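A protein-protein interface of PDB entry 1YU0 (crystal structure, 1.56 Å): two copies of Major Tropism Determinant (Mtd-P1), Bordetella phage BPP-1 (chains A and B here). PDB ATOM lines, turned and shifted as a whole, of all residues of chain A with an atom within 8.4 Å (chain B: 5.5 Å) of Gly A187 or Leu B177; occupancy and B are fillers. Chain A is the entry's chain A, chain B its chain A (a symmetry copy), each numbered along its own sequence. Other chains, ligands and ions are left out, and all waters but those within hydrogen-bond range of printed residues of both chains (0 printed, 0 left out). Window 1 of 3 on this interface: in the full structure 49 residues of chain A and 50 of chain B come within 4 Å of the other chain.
The side-chain amino group of Lys B224 lies within hydrogen-bond range of the backbone carbonyl oxygen of Ala A186 (3.0 Å).
OG1 of Thr A183 lies within hydrogen-bond range of O of Trp A297 (2.7 Å).
O of Gly A187 sits at hydrogen-bond distance from ND1 of His A377, at 3.3 Å.
The backbone carbonyl oxygen (O) of His B248 is in hydrogen-bond range of the backbone NH (N) of Leu B177 (3.3 Å).
The backbone carbonyl oxygen of His B247 is in hydrogen-bond range of the side-chain amino group of Lys B224 (2.8 Å).
Among the printed residues, merely in contact across the chains: Ala A186 with Thr B246, Ala A186 with His B247, Gly A187 with Leu B177, Ala A188 with Thr B246 and Trp A297 with Lys B224.
Gly A187 touches just one residue of chain B: Leu B177.
Of chain A, only Gly A187 comes within 4 Å of Leu B177.
No residue of chain A comes within 4 Å of Ala B176.
Of the printed residues of chain A, His B247 touches Ala A186 (3.9 Å).
Of the printed residues of chain B, Trp A297 touches Lys B224.
Of the printed residues of chain B, Ala A186 touches Lys B224 (3.0 Å), Thr B246 (3.9 Å) and His B247 (3.9 Å).
Of the printed residues of chain A, Lys B224 touches Ala A186 (3.0 Å) and Trp A297 (3.6 Å).
Thr A183 touches none of the printed residues of chain B.
Gly B249 touches none of the printed residues of chain A.
The nearest residue of chain B that does not touch Gly A187 is Lys B224 (4.6 Å).
The nearest residue of chain A that does not touch Leu B177 is Ala A186 (4.1 Å).
The nearest printed residue of chain A that does not touch His B247 is Ala A188 (5.6 Å).
Of the 16 printed residues of chain A, 4 touch a printed residue of chain B.
Hydrophobic or aromatic side chains of chain A within 4 Å of the printed part of chain B: Ala A188 and Trp A297.
Hydrophobic or aromatic side chains of chain B that line the printed part of chain A: Leu B177.
No position is printed for both chains.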
ATOM      1  N   SER A  63      29.747   5.003  -1.848  1.00  0.00           N
ATOM      2  CA  SER A  63      28.635   4.940  -2.802  1.00  0.00           C
ATOM      3  C   SER A  63      27.264   4.797  -2.148  1.00  0.00           C
ATOM      4  O   SER A  63      26.253   4.719  -2.844  1.00  0.00           O
ATOM      5  CB  SER A  63      28.841   3.788  -3.779  1.00  0.00           C
ATOM      6  OG  SER A  63      28.501   2.542  -3.185  1.00  0.00           O
ATOM      7  N   TYR A 165      14.895   5.798   2.386  1.00  0.00           N
ATOM      8  CA  TYR A 165      15.409   6.494   1.207  1.00  0.00           C
ATOM      9  C   TYR A 165      15.605   7.979   1.441  1.00  0.00           C
ATOM     10  O   TYR A 165      16.210   8.665   0.615  1.00  0.00           O
ATOM     11  CB  TYR A 165      14.486   6.259   0.016  1.00  0.00           C
ATOM     12  CG  TYR A 165      14.375   4.811  -0.392  1.00  0.00           C
ATOM     13  CD1 TYR A 165      15.484   4.111  -0.853  1.00  0.00           C
ATOM     14  CD2 TYR A 165      13.161   4.135  -0.319  1.00  0.00           C
ATOM     15  CE1 TYR A 165      15.381   2.790  -1.234  1.00  0.00           C
ATOM     16  CE2 TYR A 165      13.056   2.823  -0.712  1.00  0.00           C
ATOM     17  CZ  TYR A 165      14.162   2.154  -1.166  1.00  0.00           C
ATOM     18  OH  TYR A 165      14.079   0.823  -1.570  1.00  0.00           O
ATOM     19  N   PHE A 172      26.423  12.428   0.635  1.00  0.00           N
ATOM     20  CA  PHE A 172      25.437  11.578  -0.085  1.00  0.00           C
ATOM     21  C   PHE A 172      24.076  12.214   0.124  1.00  0.00           C
ATOM     22  O   PHE A 172      23.437  12.001   1.149  1.00  0.00           O
ATOM     23  CB  PHE A 172      25.504  10.157   0.483  1.00  0.00           C
ATOM     24  CG  PHE A 172      24.651   9.150  -0.238  1.00  0.00           C
ATOM     25  CD1 PHE A 172      25.202   8.309  -1.197  1.00  0.00           C
ATOM     26  CD2 PHE A 172      23.293   9.032   0.052  1.00  0.00           C
ATOM     27  CE1 PHE A 172      24.417   7.366  -1.854  1.00  0.00           C
ATOM     28  CE2 PHE A 172      22.506   8.091  -0.600  1.00  0.00           C
ATOM     29  CZ  PHE A 172      23.066   7.249  -1.536  1.00  0.00           C
ATOM     30  N   THR A 183      13.589  12.610  -0.729  1.00  0.00           N
ATOM     31  CA  THR A 183      13.876  11.193  -0.774  1.00  0.00           C
ATOM     32  C   THR A 183      14.603  10.803  -2.067  1.00  0.00           C
ATOM     33  O   THR A 183      14.390  11.386  -3.124  1.00  0.00           O
ATOM     34  CB  THR A 183      12.590  10.370  -0.617  1.00  0.00           C
ATOM     35  OG1 THR A 183      12.934   8.997  -0.468  1.00  0.00           O
ATOM     36  CG2 THR A 183      11.640  10.570  -1.782  1.00  0.00           C
ATOM     37  N   LEU A 184      15.466   9.804  -1.954  1.00  0.00           N
ATOM     38  CA  LEU A 184      16.286   9.361  -3.072  1.00  0.00           C
ATOM     39  C   LEU A 184      15.545   8.295  -3.851  1.00  0.00           C
ATOM     40  O   LEU A 184      15.212   7.244  -3.322  1.00  0.00           O
ATOM     41  CB  LEU A 184      17.615   8.809  -2.556  1.00  0.00           C
ATOM     42  CG  LEU A 184      18.622   8.341  -3.601  1.00  0.00           C
ATOM     43  CD1 LEU A 184      18.972   9.442  -4.585  1.00  0.00           C
ATOM     44  CD2 LEU A 184      19.868   7.813  -2.890  1.00  0.00           C
ATOM     45  N   VAL A 185      15.324   8.580  -5.121  1.00  0.00           N
ATOM     46  CA  VAL A 185      14.575   7.731  -6.037  1.00  0.00           C
ATOM     47  C   VAL A 185      15.515   6.860  -6.856  1.00  0.00           C
ATOM     48  O   VAL A 185      16.289   7.355  -7.673  1.00  0.00           O
ATOM     49  CB  VAL A 185      13.726   8.602  -6.990  1.00  0.00           C
ATOM     50  CG1 VAL A 185      12.995   7.751  -8.014  1.00  0.00           C
ATOM     51  CG2 VAL A 185      12.768   9.489  -6.215  1.00  0.00           C
ATOM     52  N   ALA A 186      15.455   5.553  -6.615  1.00  0.00           N
ATOM     53  CA  ALA A 186      16.227   4.554  -7.360  1.00  0.00           C
ATOM     54  C   ALA A 186      17.731   4.785  -7.330  1.00  0.00           C
ATOM     55  O   ALA A 186      18.453   4.329  -8.221  1.00  0.00           O
ATOM     56  CB  ALA A 186      15.720   4.457  -8.821  1.00  0.00           C
ATOM     57  N   GLY A 187      18.212   5.503  -6.312  1.00  0.00           N
ATOM     58  CA  GLY A 187      19.621   5.874  -6.203  1.00  0.00           C
ATOM     59  C   GLY A 187      20.084   6.913  -7.198  1.00  0.00           C
ATOM     60  O   GLY A 187      21.285   7.189  -7.290  1.00  0.00           O
ATOM     61  N   ALA A 188      19.140   7.523  -7.916  1.00  0.00           N
ATOM     62  CA  ALA A 188      19.433   8.324  -9.117  1.00  0.00           C
ATOM     63  C   ALA A 188      19.282   9.843  -8.979  1.00  0.00           C
ATOM     64  O   ALA A 188      20.050  10.591  -9.570  1.00  0.00           O
ATOM     65  CB  ALA A 188      18.572   7.831 -10.259  1.00  0.00           C
ATOM     66  N   PHE A 189      18.245  10.288  -8.283  1.00  0.00           N
ATOM     67  CA  PHE A 189      17.953  11.699  -8.091  1.00  0.00           C
ATOM     68  C   PHE A 189      17.018  11.810  -6.886  1.00  0.00           C
ATOM     69  O   PHE A 189      16.457  10.804  -6.460  1.00  0.00           O
ATOM     70  CB  PHE A 189      17.298  12.314  -9.343  1.00  0.00           C
ATOM     71  CG  PHE A 189      15.895  11.815  -9.610  1.00  0.00           C
ATOM     72  CD1 PHE A 189      14.790  12.493  -9.103  1.00  0.00           C
ATOM     73  CD2 PHE A 189      15.679  10.662 -10.330  1.00  0.00           C
ATOM     74  CE1 PHE A 189      13.507  12.027  -9.319  1.00  0.00           C
ATOM     75  CE2 PHE A 189      14.383  10.178 -10.531  1.00  0.00           C
ATOM     76  CZ  PHE A 189      13.302  10.882 -10.021  1.00  0.00           C
ATOM     77  N   TRP A 190      16.838  13.016  -6.359  1.00  0.00           N
ATOM     78  CA  TRP A 190      15.976  13.232  -5.182  1.00  0.00           C
ATOM     79  C   TRP A 190      14.676  13.928  -5.565  1.00  0.00           C
ATOM     80  O   TRP A 190      14.643  14.774  -6.461  1.00  0.00           O
ATOM     81  CB  TRP A 190      16.680  14.044  -4.100  1.00  0.00           C
ATOM     82  CG  TRP A 190      17.907  13.400  -3.546  1.00  0.00           C
ATOM     83  CD1 TRP A 190      19.099  13.243  -4.186  1.00  0.00           C
ATOM     84  CD2 TRP A 190      18.070  12.777  -2.255  1.00  0.00           C
ATOM     85  NE1 TRP A 190      19.995  12.607  -3.377  1.00  0.00           N
ATOM     86  CE2 TRP A 190      19.395  12.300  -2.182  1.00  0.00           C
ATOM     87  CE3 TRP A 190      17.235  12.609  -1.144  1.00  0.00           C
ATOM     88  CZ2 TRP A 190      19.895  11.630  -1.049  1.00  0.00           C
ATOM     89  CZ3 TRP A 190      17.738  11.965  -0.022  1.00  0.00           C
ATOM     90  CH2 TRP A 190      19.049  11.485   0.017  1.00  0.00           C
ATOM     91  N   TRP A 297       9.364   5.074  -2.905  1.00  0.00           N
ATOM     92  CA  TRP A 297      10.423   5.901  -2.337  1.00  0.00           C
ATOM     93  C   TRP A 297       9.896   6.776  -1.199  1.00  0.00           C
ATOM     94  O   TRP A 297      10.657   7.548  -0.609  1.00  0.00           O
ATOM     95  CB  TRP A 297      11.084   6.749  -3.454  1.00  0.00           C
ATOM     96  CG  TRP A 297      11.238   5.973  -4.703  1.00  0.00           C
ATOM     97  CD1 TRP A 297      10.489   6.088  -5.845  1.00  0.00           C
ATOM     98  CD2 TRP A 297      12.127   4.869  -4.921  1.00  0.00           C
ATOM     99  NE1 TRP A 297      10.866   5.138  -6.759  1.00  0.00           N
ATOM    100  CE2 TRP A 297      11.868   4.374  -6.214  1.00  0.00           C
ATOM    101  CE3 TRP A 297      13.115   4.251  -4.150  1.00  0.00           C
ATOM    102  CZ2 TRP A 297      12.585   3.312  -6.761  1.00  0.00           C
ATOM    103  CZ3 TRP A 297      13.814   3.191  -4.686  1.00  0.00           C
ATOM    104  CH2 TRP A 297      13.546   2.725  -5.977  1.00  0.00           C
ATOM    105  N   ASP A 376      19.228  16.889  -8.486  1.00  0.00           N
ATOM    106  CA  ASP A 376      20.206  15.841  -8.716  1.00  0.00           C
ATOM    107  C   ASP A 376      20.652  15.202  -7.385  1.00  0.00           C
ATOM    108  O   ASP A 376      20.476  15.773  -6.301  1.00  0.00           O
ATOM    109  CB  ASP A 376      21.442  16.416  -9.422  1.00  0.00           C
ATOM    110  CG  ASP A 376      21.204  16.780 -10.854  1.00  0.00           C
ATOM    111  OD1 ASP A 376      20.085  16.629 -11.398  1.00  0.00           O
ATOM    112  OD2 ASP A 376      22.213  17.213 -11.472  1.00  0.00           O
ATOM    113  N   HIS A 377      21.254  14.032  -7.517  1.00  0.00           N
ATOM    114  CA  HIS A 377      21.892  13.314  -6.430  1.00  0.00           C
ATOM    115  C   HIS A 377      23.376  13.657  -6.421  1.00  0.00           C
ATOM    116  O   HIS A 377      24.016  13.708  -7.479  1.00  0.00           O
ATOM    117  CB  HIS A 377      21.695  11.819  -6.648  1.00  0.00           C
ATOM    118  CG  HIS A 377      22.254  10.977  -5.555  1.00  0.00           C
ATOM    119  ND1 HIS A 377      22.684   9.681  -5.737  1.00  0.00           N
ATOM    120  CD2 HIS A 377      22.412  11.249  -4.242  1.00  0.00           C
ATOM    121  CE1 HIS A 377      23.069   9.192  -4.564  1.00  0.00           C
ATOM    122  NE2 HIS A 377      22.937  10.131  -3.655  1.00  0.00           N
ATOM    123  N   LEU A 378      23.921  13.907  -5.245  1.00  0.00           N
ATOM    124  CA  LEU A 378      25.335  14.232  -5.097  1.00  0.00           C
ATOM    125  C   LEU A 378      26.015  13.202  -4.218  1.00  0.00           C
ATOM    126  O   LEU A 378      25.623  13.020  -3.063  1.00  0.00           O
ATOM    127  CB  LEU A 378      25.476  15.608  -4.477  1.00  0.00           C
ATOM    128  CG  LEU A 378      26.902  16.101  -4.308  1.00  0.00           C
ATOM    129  CD1 LEU A 378      27.528  16.318  -5.664  1.00  0.00           C
ATOM    130  CD2 LEU A 378      26.878  17.367  -3.508  1.00  0.00           C
ATOM    131  N   ILE A 379      27.011  12.524  -4.778  1.00  0.00           N
ATOM    132  CA  ILE A 379      27.915  11.675  -4.010  1.00  0.00           C
ATOM    133  C   ILE A 379      29.321  12.263  -4.089  1.00  0.00           C
ATOM    134  O   ILE A 379      29.861  12.479  -5.195  1.00  0.00           O
ATOM    135  CB  ILE A 379      27.938  10.217  -4.512  1.00  0.00           C
ATOM    136  CG1 ILE A 379      26.507   9.657  -4.629  1.00  0.00           C
ATOM    137  CG2 ILE A 379      28.725   9.367  -3.537  1.00  0.00           C
ATOM    138  CD1 ILE A 379      26.457   8.182  -4.977  1.00  0.00           C
ATOM    139  N   ALA B 175      28.891  10.659 -13.223  1.00  0.00           N
ATOM    140  CA  ALA B 175      27.887  10.727 -12.152  1.00  0.00           C
ATOM    141  C   ALA B 175      26.807   9.720 -12.472  1.00  0.00           C
ATOM    142  O   ALA B 175      25.675  10.102 -12.823  1.00  0.00           O
ATOM    143  CB  ALA B 175      27.304  12.126 -12.084  1.00  0.00           C
ATOM    144  N   ALA B 176      27.195   8.460 -12.497  1.00  0.00           N
ATOM    145  CA  ALA B 176      26.305   7.310 -12.630  1.00  0.00           C
ATOM    146  C   ALA B 176      26.688   6.344 -11.549  1.00  0.00           C
ATOM    147  O   ALA B 176      27.726   6.478 -10.915  1.00  0.00           O
ATOM    148  CB  ALA B 176      26.466   6.641 -13.971  1.00  0.00           C
ATOM    149  N   LEU B 177      25.852   5.337 -11.336  1.00  0.00           N
ATOM    150  CA  LEU B 177      26.067   4.450 -10.208  1.00  0.00           C
ATOM    151  C   LEU B 177      27.294   3.556 -10.379  1.00  0.00           C
ATOM    152  O   LEU B 177      27.851   3.103  -9.390  1.00  0.00           O
ATOM    153  CB  LEU B 177      24.815   3.624  -9.929  1.00  0.00           C
ATOM    154  CG  LEU B 177      23.597   4.485  -9.588  1.00  0.00           C
ATOM    155  CD1 LEU B 177      22.442   3.622  -9.113  1.00  0.00           C
ATOM    156  CD2 LEU B 177      23.942   5.583  -8.582  1.00  0.00           C
ATOM    157  N   ASP B 178      27.730   3.346 -11.613  1.00  0.00           N
ATOM    158  CA  ASP B 178      28.950   2.576 -11.916  1.00  0.00           C
ATOM    159  C   ASP B 178      29.604   3.237 -13.118  1.00  0.00           C
ATOM    160  O   ASP B 178      28.907   3.581 -14.072  1.00  0.00           O
ATOM    161  CB  ASP B 178      28.578   1.133 -12.233  1.00  0.00           C
ATOM    162  CG  ASP B 178      29.766   0.209 -12.228  1.00  0.00           C
ATOM    163  OD1 ASP B 178      30.547   0.259 -13.182  1.00  0.00           O
ATOM    164  OD2 ASP B 178      29.925  -0.555 -11.256  1.00  0.00           O
ATOM    165  N   PRO B 179      30.934   3.430 -13.099  1.00  0.00           N
ATOM    166  CA  PRO B 179      31.604   4.109 -14.208  1.00  0.00           C
ATOM    167  C   PRO B 179      31.958   3.241 -15.413  1.00  0.00           C
ATOM    168  O   PRO B 179      32.353   3.772 -16.456  1.00  0.00           O
ATOM    169  CB  PRO B 179      32.878   4.632 -13.557  1.00  0.00           C
ATOM    170  CG  PRO B 179      33.209   3.569 -12.575  1.00  0.00           C
ATOM    171  CD  PRO B 179      31.875   3.133 -12.007  1.00  0.00           C
ATOM    172  N   LYS B 224      14.552  -2.417  -9.389  1.00  0.00           N
ATOM    173  CA  LYS B 224      14.146  -1.262  -8.575  1.00  0.00           C
ATOM    174  C   LYS B 224      12.705  -0.843  -8.848  1.00  0.00           C
ATOM    175  O   LYS B 224      12.162  -0.010  -8.112  1.00  0.00           O
ATOM    176  CB  LYS B 224      15.091  -0.070  -8.798  1.00  0.00           C
ATOM    177  CG  LYS B 224      16.488  -0.309  -8.258  1.00  0.00           C
ATOM    178  CD  LYS B 224      17.429   0.848  -8.530  1.00  0.00           C
ATOM    179  CE  LYS B 224      18.839   0.532  -8.110  1.00  0.00           C
ATOM    180  NZ  LYS B 224      19.795   1.659  -8.355  1.00  0.00           N
ATOM    181  N   THR B 246      17.227   5.029 -15.429  1.00  0.00           N
ATOM    182  CA  THR B 246      17.119   5.549 -14.063  1.00  0.00           C
ATOM    183  C   THR B 246      17.675   4.549 -13.045  1.00  0.00           C
ATOM    184  O   THR B 246      18.400   4.931 -12.123  1.00  0.00           O
ATOM    185  CB  THR B 246      15.668   5.911 -13.739  1.00  0.00           C
ATOM    186  OG1 THR B 246      15.229   6.903 -14.673  1.00  0.00           O
ATOM    187  CG2 THR B 246      15.544   6.451 -12.330  1.00  0.00           C
ATOM    188  N   HIS B 247      17.351   3.270 -13.227  1.00  0.00           N
ATOM    189  CA  HIS B 247      17.882   2.208 -12.367  1.00  0.00           C
ATOM    190  C   HIS B 247      19.390   2.331 -12.191  1.00  0.00           C
ATOM    191  O   HIS B 247      19.922   2.121 -11.102  1.00  0.00           O
ATOM    192  CB  HIS B 247      17.558   0.867 -13.015  1.00  0.00           C
ATOM    193  CG  HIS B 247      18.045  -0.330 -12.269  1.00  0.00           C
ATOM    194  ND1 HIS B 247      19.374  -0.689 -12.162  1.00  0.00           N
ATOM    195  CD2 HIS B 247      17.344  -1.317 -11.673  1.00  0.00           C
ATOM    196  CE1 HIS B 247      19.463  -1.838 -11.501  1.00  0.00           C
ATOM    197  NE2 HIS B 247      18.244  -2.228 -11.182  1.00  0.00           N
ATOM    198  N   HIS B 248      20.081   2.667 -13.275  1.00  0.00           N
ATOM    199  CA  HIS B 248      21.537   2.716 -13.283  1.00  0.00           C
ATOM    200  C   HIS B 248      22.106   4.111 -13.042  1.00  0.00           C
ATOM    201  O   HIS B 248      23.313   4.328 -13.164  1.00  0.00           O
ATOM    202  CB  HIS B 248      22.012   2.147 -14.619  1.00  0.00           C
ATOM    203  CG  HIS B 248      21.811   0.668 -14.736  1.00  0.00           C
ATOM    204  ND1 HIS B 248      20.738   0.078 -15.374  1.00  0.00           N
ATOM    205  CD2 HIS B 248      22.562  -0.346 -14.252  1.00  0.00           C
ATOM    206  CE1 HIS B 248      20.851  -1.238 -15.281  1.00  0.00           C
ATOM    207  NE2 HIS B 248      21.952  -1.518 -14.610  1.00  0.00           N
ATOM    208  N   GLY B 249      21.253   5.068 -12.685  1.00  0.00           N
ATOM    209  CA  GLY B 249      21.710   6.436 -12.473  1.00  0.00           C
ATOM    210  C   GLY B 249      22.106   7.164 -13.741  1.00  0.00           C
ATOM    211  O   GLY B 249      22.999   8.023 -13.731  1.00  0.00           O
